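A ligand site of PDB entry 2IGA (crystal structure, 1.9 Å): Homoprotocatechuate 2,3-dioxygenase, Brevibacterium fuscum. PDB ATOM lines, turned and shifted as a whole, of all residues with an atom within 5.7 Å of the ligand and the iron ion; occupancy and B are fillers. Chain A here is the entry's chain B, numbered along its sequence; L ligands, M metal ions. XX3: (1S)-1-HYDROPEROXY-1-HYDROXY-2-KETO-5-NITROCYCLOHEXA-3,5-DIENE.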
ATOM      1  N   HIS A 155       8.779   9.356   8.783  1.00  0.00           N
ATOM      2  CA  HIS A 155       9.335  10.247   9.784  1.00  0.00           C
ATOM      3  C   HIS A 155      10.175  11.341   9.180  1.00  0.00           C
ATOM      4  O   HIS A 155      10.488  11.307   8.013  1.00  0.00           O
ATOM      5  CB  HIS A 155      10.159   9.506  10.860  1.00  0.00           C
ATOM      6  CG  HIS A 155      11.364   8.753  10.350  1.00  0.00           C
ATOM      7  ND1 HIS A 155      11.297   7.431   9.935  1.00  0.00           N
ATOM      8  CD2 HIS A 155      12.667   9.136  10.180  1.00  0.00           C
ATOM      9  CE1 HIS A 155      12.505   7.034   9.561  1.00  0.00           C
ATOM     10  NE2 HIS A 155      13.353   8.038   9.700  1.00  0.00           N
ATOM     11  N   PHE A 156      10.484  12.306  10.031  1.00  0.00           N
ATOM     12  CA  PHE A 156      11.544  13.285   9.781  1.00  0.00           C
ATOM     13  C   PHE A 156      12.733  12.962  10.709  1.00  0.00           C
ATOM     14  O   PHE A 156      12.604  12.189  11.672  1.00  0.00           O
ATOM     15  CB  PHE A 156      11.008  14.688  10.072  1.00  0.00           C
ATOM     16  CG  PHE A 156       9.678  14.989   9.458  1.00  0.00           C
ATOM     17  CD1 PHE A 156       9.455  14.816   8.102  1.00  0.00           C
ATOM     18  CD2 PHE A 156       8.626  15.482  10.246  1.00  0.00           C
ATOM     19  CE1 PHE A 156       8.197  15.127   7.515  1.00  0.00           C
ATOM     20  CE2 PHE A 156       7.400  15.800   9.678  1.00  0.00           C
ATOM     21  CZ  PHE A 156       7.186  15.623   8.313  1.00  0.00           C
ATOM     22  N   ASN A 157      13.875  13.586  10.432  1.00  0.00           N
ATOM     23  CA  ASN A 157      15.012  13.551  11.310  1.00  0.00           C
ATOM     24  C   ASN A 157      15.678  14.904  11.272  1.00  0.00           C
ATOM     25  O   ASN A 157      16.008  15.402  10.184  1.00  0.00           O
ATOM     26  CB  ASN A 157      15.988  12.456  10.926  1.00  0.00           C
ATOM     27  CG  ASN A 157      17.022  12.210  12.009  1.00  0.00           C
ATOM     28  OD1 ASN A 157      17.761  13.139  12.403  1.00  0.00           O
ATOM     29  ND2 ASN A 157      17.089  10.966  12.498  1.00  0.00           N
ATOM     30  N   ILE A 181      20.637   7.333  21.920  1.00  0.00           N
ATOM     31  CA  ILE A 181      22.049   7.007  21.979  1.00  0.00           C
ATOM     32  C   ILE A 181      22.757   7.950  22.964  1.00  0.00           C
ATOM     33  O   ILE A 181      22.650   9.197  22.882  1.00  0.00           O
ATOM     34  CB  ILE A 181      22.695   7.071  20.555  1.00  0.00           C
ATOM     35  CG1 ILE A 181      22.122   5.931  19.674  1.00  0.00           C
ATOM     36  CG2 ILE A 181      24.190   6.931  20.667  1.00  0.00           C
ATOM     37  CD1 ILE A 181      22.317   6.156  18.201  1.00  0.00           C
ATOM     38  N   TRP A 192      14.956   9.328  19.493  1.00  0.00           N
ATOM     39  CA  TRP A 192      13.818   8.971  18.583  1.00  0.00           C
ATOM     40  C   TRP A 192      12.478   9.134  19.335  1.00  0.00           C
ATOM     41  O   TRP A 192      12.383   8.737  20.511  1.00  0.00           O
ATOM     42  CB  TRP A 192      13.941   7.511  18.108  1.00  0.00           C
ATOM     43  CG  TRP A 192      14.976   7.268  17.025  1.00  0.00           C
ATOM     44  CD1 TRP A 192      14.740   6.997  15.691  1.00  0.00           C
ATOM     45  CD2 TRP A 192      16.420   7.300  17.184  1.00  0.00           C
ATOM     46  NE1 TRP A 192      15.947   6.881  15.035  1.00  0.00           N
ATOM     47  CE2 TRP A 192      16.988   7.074  15.911  1.00  0.00           C
ATOM     48  CE3 TRP A 192      17.270   7.538  18.281  1.00  0.00           C
ATOM     49  CZ2 TRP A 192      18.394   7.029  15.705  1.00  0.00           C
ATOM     50  CZ3 TRP A 192      18.676   7.478  18.082  1.00  0.00           C
ATOM     51  CH2 TRP A 192      19.204   7.224  16.802  1.00  0.00           C
ATOM     52  N   HIS A 200       9.285   6.231  15.390  1.00  0.00           N
ATOM     53  CA  HIS A 200       9.245   7.692  15.426  1.00  0.00           C
ATOM     54  C   HIS A 200       8.327   8.406  14.426  1.00  0.00           C
ATOM     55  O   HIS A 200       8.006   7.841  13.407  1.00  0.00           O
ATOM     56  CB  HIS A 200      10.674   8.290  15.436  1.00  0.00           C
ATOM     57  CG  HIS A 200      11.541   7.848  14.293  1.00  0.00           C
ATOM     58  ND1 HIS A 200      11.517   6.565  13.767  1.00  0.00           N
ATOM     59  CD2 HIS A 200      12.520   8.514  13.626  1.00  0.00           C
ATOM     60  CE1 HIS A 200      12.431   6.462  12.824  1.00  0.00           C
ATOM     61  NE2 HIS A 200      13.073   7.617  12.734  1.00  0.00           N
ATOM     62  N   ALA A 203      12.939  12.704  15.065  1.00  0.00           N
ATOM     63  CA  ALA A 203      14.064  12.299  15.847  1.00  0.00           C
ATOM     64  C   ALA A 203      15.019  13.484  15.874  1.00  0.00           C
ATOM     65  O   ALA A 203      14.961  14.346  14.976  1.00  0.00           O
ATOM     66  CB  ALA A 203      14.719  11.015  15.273  1.00  0.00           C
ATOM     67  N   THR A 205      19.097  14.460  15.866  1.00  0.00           N
ATOM     68  CA  THR A 205      20.461  14.011  15.655  1.00  0.00           C
ATOM     69  C   THR A 205      21.355  15.131  16.076  1.00  0.00           C
ATOM     70  O   THR A 205      21.282  16.246  15.524  1.00  0.00           O
ATOM     71  CB  THR A 205      20.751  13.678  14.166  1.00  0.00           C
ATOM     72  OG1 THR A 205      19.936  12.581  13.773  1.00  0.00           O
ATOM     73  CG2 THR A 205      22.192  13.269  13.952  1.00  0.00           C
ATOM     74  N   HIS A 214      16.885  14.302   7.309  1.00  0.00           N
ATOM     75  CA  HIS A 214      16.256  13.560   6.227  1.00  0.00           C
ATOM     76  C   HIS A 214      14.749  13.448   6.445  1.00  0.00           C
ATOM     77  O   HIS A 214      14.254  13.772   7.556  1.00  0.00           O
ATOM     78  CB  HIS A 214      16.892  12.151   6.043  1.00  0.00           C
ATOM     79  CG  HIS A 214      16.810  11.242   7.258  1.00  0.00           C
ATOM     80  ND1 HIS A 214      17.820  11.140   8.207  1.00  0.00           N
ATOM     81  CD2 HIS A 214      15.831  10.390   7.659  1.00  0.00           C
ATOM     82  CE1 HIS A 214      17.448  10.274   9.144  1.00  0.00           C
ATOM     83  NE2 HIS A 214      16.259   9.807   8.830  1.00  0.00           N
ATOM     84  N   ALA A 216      11.853  10.340   5.643  1.00  0.00           N
ATOM     85  CA  ALA A 216      11.815   8.902   5.397  1.00  0.00           C
ATOM     86  C   ALA A 216      10.498   8.396   4.885  1.00  0.00           C
ATOM     87  O   ALA A 216       9.436   8.714   5.446  1.00  0.00           O
ATOM     88  CB  ALA A 216      12.164   8.101   6.696  1.00  0.00           C
ATOM     89  N   ARG A 243      24.466   5.877   1.718  1.00  0.00           N
ATOM     90  CA  ARG A 243      24.804   4.950   2.786  1.00  0.00           C
ATOM     91  C   ARG A 243      23.719   3.865   2.823  1.00  0.00           C
ATOM     92  O   ARG A 243      22.522   4.173   2.749  1.00  0.00           O
ATOM     93  CB  ARG A 243      24.823   5.679   4.163  1.00  0.00           C
ATOM     94  CG  ARG A 243      24.583   4.708   5.328  1.00  0.00           C
ATOM     95  CD  ARG A 243      24.678   5.337   6.724  1.00  0.00           C
ATOM     96  NE  ARG A 243      24.444   4.299   7.723  1.00  0.00           N
ATOM     97  CZ  ARG A 243      23.805   4.447   8.885  1.00  0.00           C
ATOM     98  NH1 ARG A 243      23.291   5.623   9.249  1.00  0.00           N
ATOM     99  NH2 ARG A 243      23.653   3.386   9.649  1.00  0.00           N
ATOM    100  N   HIS A 248      19.162  -1.262  10.706  1.00  0.00           N
ATOM    101  CA  HIS A 248      19.455  -0.380  11.814  1.00  0.00           C
ATOM    102  C   HIS A 248      19.520  -1.216  13.134  1.00  0.00           C
ATOM    103  O   HIS A 248      18.824  -2.205  13.283  1.00  0.00           O
ATOM    104  CB  HIS A 248      18.293   0.642  11.977  1.00  0.00           C
ATOM    105  CG  HIS A 248      18.385   1.840  11.077  1.00  0.00           C
ATOM    106  ND1 HIS A 248      19.555   2.520  10.856  1.00  0.00           N
ATOM    107  CD2 HIS A 248      17.446   2.459  10.334  1.00  0.00           C
ATOM    108  CE1 HIS A 248      19.318   3.530  10.025  1.00  0.00           C
ATOM    109  NE2 HIS A 248      18.034   3.528   9.727  1.00  0.00           N
ATOM    110  N   GLY A 249      20.341  -0.793  14.104  1.00  0.00           N
ATOM    111  CA  GLY A 249      20.201  -1.237  15.468  1.00  0.00           C
ATOM    112  C   GLY A 249      18.991  -0.493  16.031  1.00  0.00           C
ATOM    113  O   GLY A 249      17.891  -1.080  16.238  1.00  0.00           O
ATOM    114  N   VAL A 250      19.206   0.803  16.280  1.00  0.00           N
ATOM    115  CA  VAL A 250      18.140   1.645  16.786  1.00  0.00           C
ATOM    116  C   VAL A 250      17.004   1.535  15.793  1.00  0.00           C
ATOM    117  O   VAL A 250      17.176   1.760  14.618  1.00  0.00           O
ATOM    118  CB  VAL A 250      18.589   3.100  16.880  1.00  0.00           C
ATOM    119  CG1 VAL A 250      17.402   4.018  16.991  1.00  0.00           C
ATOM    120  CG2 VAL A 250      19.557   3.278  18.019  1.00  0.00           C
ATOM    121  N   SER A 251      15.825   1.118  16.267  1.00  0.00           N
ATOM    122  CA  SER A 251      14.650   0.973  15.423  1.00  0.00           C
ATOM    123  C   SER A 251      14.469  -0.387  14.813  1.00  0.00           C
ATOM    124  O   SER A 251      13.352  -0.756  14.537  1.00  0.00           O
ATOM    125  CB  SER A 251      14.517   2.046  14.338  1.00  0.00           C
ATOM    126  OG  SER A 251      15.158   1.695  13.102  1.00  0.00           O
ATOM    127  N   TYR A 257      19.867   5.248   2.587  1.00  0.00           N
ATOM    128  CA  TYR A 257      19.887   6.696   2.425  1.00  0.00           C
ATOM    129  C   TYR A 257      20.385   7.188   1.002  1.00  0.00           C
ATOM    130  O   TYR A 257      21.429   6.795   0.584  1.00  0.00           O
ATOM    131  CB  TYR A 257      20.784   7.354   3.502  1.00  0.00           C
ATOM    132  CG  TYR A 257      20.343   7.040   4.902  1.00  0.00           C
ATOM    133  CD1 TYR A 257      19.330   7.804   5.520  1.00  0.00           C
ATOM    134  CD2 TYR A 257      20.967   6.017   5.626  1.00  0.00           C
ATOM    135  CE1 TYR A 257      18.927   7.499   6.815  1.00  0.00           C
ATOM    136  CE2 TYR A 257      20.583   5.716   6.960  1.00  0.00           C
ATOM    137  CZ  TYR A 257      19.558   6.474   7.505  1.00  0.00           C
ATOM    138  OH  TYR A 257      19.191   6.207   8.787  1.00  0.00           O
ATOM    139  N   GLU A 267      15.515   8.913   3.282  1.00  0.00           N
ATOM    140  CA  GLU A 267      15.635   7.555   3.802  1.00  0.00           C
ATOM    141  C   GLU A 267      14.501   6.707   3.295  1.00  0.00           C
ATOM    142  O   GLU A 267      13.342   7.153   3.238  1.00  0.00           O
ATOM    143  CB  GLU A 267      15.531   7.503   5.331  1.00  0.00           C
ATOM    144  CG  GLU A 267      15.954   6.105   5.905  1.00  0.00           C
ATOM    145  CD  GLU A 267      15.955   6.073   7.415  1.00  0.00           C
ATOM    146  OE1 GLU A 267      15.713   7.120   8.034  1.00  0.00           O
ATOM    147  OE2 GLU A 267      16.238   5.011   7.987  1.00  0.00           O
ATOM    148  N   TYR A 269      12.736   2.952   4.280  1.00  0.00           N
ATOM    149  CA  TYR A 269      12.632   2.411   5.641  1.00  0.00           C
ATOM    150  C   TYR A 269      11.551   1.357   5.648  1.00  0.00           C
ATOM    151  O   TYR A 269      10.515   1.555   4.989  1.00  0.00           O
ATOM    152  CB  TYR A 269      12.179   3.589   6.548  1.00  0.00           C
ATOM    153  CG  TYR A 269      12.086   3.399   8.077  1.00  0.00           C
ATOM    154  CD1 TYR A 269      13.192   3.632   8.905  1.00  0.00           C
ATOM    155  CD2 TYR A 269      10.870   3.072   8.684  1.00  0.00           C
ATOM    156  CE1 TYR A 269      13.123   3.523  10.262  1.00  0.00           C
ATOM    157  CE2 TYR A 269      10.790   2.944  10.069  1.00  0.00           C
ATOM    158  CZ  TYR A 269      11.926   3.196  10.856  1.00  0.00           C
ATOM    159  OH  TYR A 269      11.845   3.084  12.234  1.00  0.00           O
ATOM    160  N   ARG A 292      24.922  -0.317  16.767  1.00  0.00           N
ATOM    161  CA  ARG A 292      23.816   0.601  17.068  1.00  0.00           C
ATOM    162  C   ARG A 292      23.178   1.320  15.852  1.00  0.00           C
ATOM    163  O   ARG A 292      21.983   1.584  15.853  1.00  0.00           O
ATOM    164  CB  ARG A 292      24.255   1.644  18.092  1.00  0.00           C
ATOM    165  CG  ARG A 292      24.928   2.888  17.374  1.00  0.00           C
ATOM    166  CD  ARG A 292      25.738   3.816  18.300  1.00  0.00           C
ATOM    167  NE  ARG A 292      26.429   4.819  17.478  1.00  0.00           N
ATOM    168  CZ  ARG A 292      27.494   4.611  16.708  1.00  0.00           C
ATOM    169  NH1 ARG A 292      28.120   3.414  16.661  1.00  0.00           N
ATOM    170  NH2 ARG A 292      27.951   5.632  15.957  1.00  0.00           N
ATOM    171  N   ARG A 293      23.960   1.655  14.837  1.00  0.00           N
ATOM    172  CA  ARG A 293      23.416   2.365  13.690  1.00  0.00           C
ATOM    173  C   ARG A 293      23.217   1.400  12.514  1.00  0.00           C
ATOM    174  O   ARG A 293      22.136   1.362  11.963  1.00  0.00           O
ATOM    175  CB  ARG A 293      24.289   3.552  13.301  1.00  0.00           C
ATOM    176  CG  ARG A 293      24.018   4.758  14.264  1.00  0.00           C
ATOM    177  CD  ARG A 293      24.383   6.063  13.638  1.00  0.00           C
ATOM    178  NE  ARG A 293      24.179   7.156  14.595  1.00  0.00           N
ATOM    179  CZ  ARG A 293      23.047   7.833  14.736  1.00  0.00           C
ATOM    180  NH1 ARG A 293      22.000   7.528  13.991  1.00  0.00           N
ATOM    181  NH2 ARG A 293      22.962   8.832  15.613  1.00  0.00           N
ATOM    182  N   ASP A 294      24.248   0.647  12.166  1.00  0.00           N
ATOM    183  CA  ASP A 294      24.132  -0.474  11.287  1.00  0.00           C
ATOM    184  C   ASP A 294      24.465  -1.737  12.122  1.00  0.00           C
ATOM    185  O   ASP A 294      25.569  -1.891  12.627  1.00  0.00           O
ATOM    186  CB  ASP A 294      25.088  -0.335  10.106  1.00  0.00           C
ATOM    187  CG  ASP A 294      24.912  -1.469   9.107  1.00  0.00           C
ATOM    188  OD1 ASP A 294      25.567  -2.522   9.246  1.00  0.00           O
ATOM    189  OD2 ASP A 294      24.063  -1.330   8.210  1.00  0.00           O
ATOM    190  N   TRP A 304      27.135  11.401   6.488  1.00  0.00           N
ATOM    191  CA  TRP A 304      25.905  11.154   7.235  1.00  0.00           C
ATOM    192  C   TRP A 304      25.941  12.055   8.486  1.00  0.00           C
ATOM    193  O   TRP A 304      24.944  12.664   8.851  1.00  0.00           O
ATOM    194  CB  TRP A 304      25.747   9.678   7.641  1.00  0.00           C
ATOM    195  CG  TRP A 304      24.313   9.323   7.898  1.00  0.00           C
ATOM    196  CD1 TRP A 304      23.362   8.970   6.965  1.00  0.00           C
ATOM    197  CD2 TRP A 304      23.612   9.395   9.170  1.00  0.00           C
ATOM    198  NE1 TRP A 304      22.141   8.788   7.585  1.00  0.00           N
ATOM    199  CE2 TRP A 304      22.261   9.044   8.924  1.00  0.00           C
ATOM    200  CE3 TRP A 304      24.021   9.731  10.491  1.00  0.00           C
ATOM    201  CZ2 TRP A 304      21.297   8.995   9.948  1.00  0.00           C
ATOM    202  CZ3 TRP A 304      23.072   9.706  11.500  1.00  0.00           C
ATOM    203  CH2 TRP A 304      21.708   9.347  11.221  1.00  0.00           C
HETATM  204  O8  XX3 L   1      17.734   7.445  10.274  1.00  0.00           O
HETATM  205  C2  XX3 L   1      17.370   7.018  11.593  1.00  0.00           C
HETATM  206  O12 XX3 L   1      16.915   8.157  12.323  1.00  0.00           O
HETATM  207  O13 XX3 L   1      15.542   8.722  11.948  1.00  0.00           O
HETATM  208  C1  XX3 L   1      16.234   5.997  11.643  1.00  0.00           C
HETATM  209  O7  XX3 L   1      15.375   5.931  10.693  1.00  0.00           O
HETATM  210  C6  XX3 L   1      16.252   5.024  12.660  1.00  0.00           C
HETATM  211  C5  XX3 L   1      17.514   4.567  13.073  1.00  0.00           C
HETATM  212  C3  XX3 L   1      18.619   6.501  12.085  1.00  0.00           C
HETATM  213  C4  XX3 L   1      18.699   5.239  12.690  1.00  0.00           C
HETATM  214  N9  XX3 L   1      19.939   4.669  12.845  1.00  0.00           N
HETATM  215  O10 XX3 L   1      21.116   5.063  12.029  1.00  0.00           O
HETATM  216  O11 XX3 L   1      19.997   3.731  13.672  1.00  0.00           O
HETATM  217 FE    FE M   1      15.566   7.921   9.879  1.00  0.00          FE
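OH of Tyr 257 lies close to O8 of the ligand, at 2.4 Å. An oxygen (O12) of the ligand is in hydrogen-bond range of the side-chain amide nitrogen (ND2) of Asn 157, at 2.8 Å. O13 of the ligand sits close to NE2 of His 200, at 2.8 Å. A ring nitrogen (ND1) of His 248 lies within hydrogen-bond range of an oxygen (O11) of the ligand, 3.1 Å away. The indole nitrogen (NE1) of Trp 192 sits close to an oxygen (O12) of the ligand, 3.1 Å away. An oxygen (O10) of the ligand sits at hydrogen-bond distance from the guanidinium group (NH1) of Arg 293, 3.3 Å away.
OE2 of Glu 267 lies within hydrogen-bond range of OH of Tyr 257 (3.3 Å). A ring nitrogen (NE2) of His 248 lies within hydrogen-bond range of the side-chain carboxylate (OE2) of Glu 267 (2.9 Å). A ring nitrogen (ND1) of His 155 lies close to a ring nitrogen (NE2) of His 200, 3.3 Å away. O of His 155 is in hydrogen-bond range of N of Ala 216, at 2.9 Å. The backbone NH of Tyr 257 sits at hydrogen-bond distance from the backbone carbonyl oxygen of Arg 243 (2.9 Å). O of Arg 293 sits at hydrogen-bond distance from ND1 of His 248 (3.0 Å). The backbone carbonyl oxygen (O) of Arg 292 is in hydrogen-bond range of the backbone NH (N) of Val 250, 2.9 Å away. The backbone carbonyl oxygen of Arg 293 is in hydrogen-bond range of the guanidinium group of Arg 243, 3.4 Å away.
Arg 243 touches the ligand. Val 250 touches the ligand (O to C5, 3.2 Å). Ser 251 touches the ligand (OG to C6, 3.5 Å). Tyr 269 touches the ligand (CE1 to O7, 3.3 Å). Arg 292 touches the ligand (O to O11, 3.6 Å). Trp 304 touches the ligand (CZ2 to O8, 3.9 Å). Hydrophobic or aromatic side chains that line the ligand: His 155, Trp 192, His 200, His 214, His 248, Val 250, Tyr 257, Tyr 269 and Trp 304. 15 residues have an atom within 4 Å of the ligand: His 155, Asn 157, Trp 192, His 200, His 214, Arg 243, His 248, Val 250, Ser 251, Tyr 257, Glu 267, Tyr 269, Arg 292, Arg 293 and Trp 304.
His 200 touches the iron ion (NE2 to FE, 3.8 Å). Within 4 Å of the iron ion: His 155, His 200, His 214 and Glu 267. The nearest printed residue that does not touch the iron ion is Tyr 257 (4.2 Å).
The iron ion is bound by OE1 of Glu 267. O7 of the ligand binds the iron ion, 2.2 Å away. O13 of the ligand is bound to the iron ion, at 2.2 Å. NE2 of His 155 binds the iron ion (2.2 Å). O8 of the ligand is bound to the iron ion, at 2.3 Å. A ring nitrogen (NE2) of His 214 is bound to the iron ion (2.3 Å). The iron ion has six donor atoms within binding distance.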
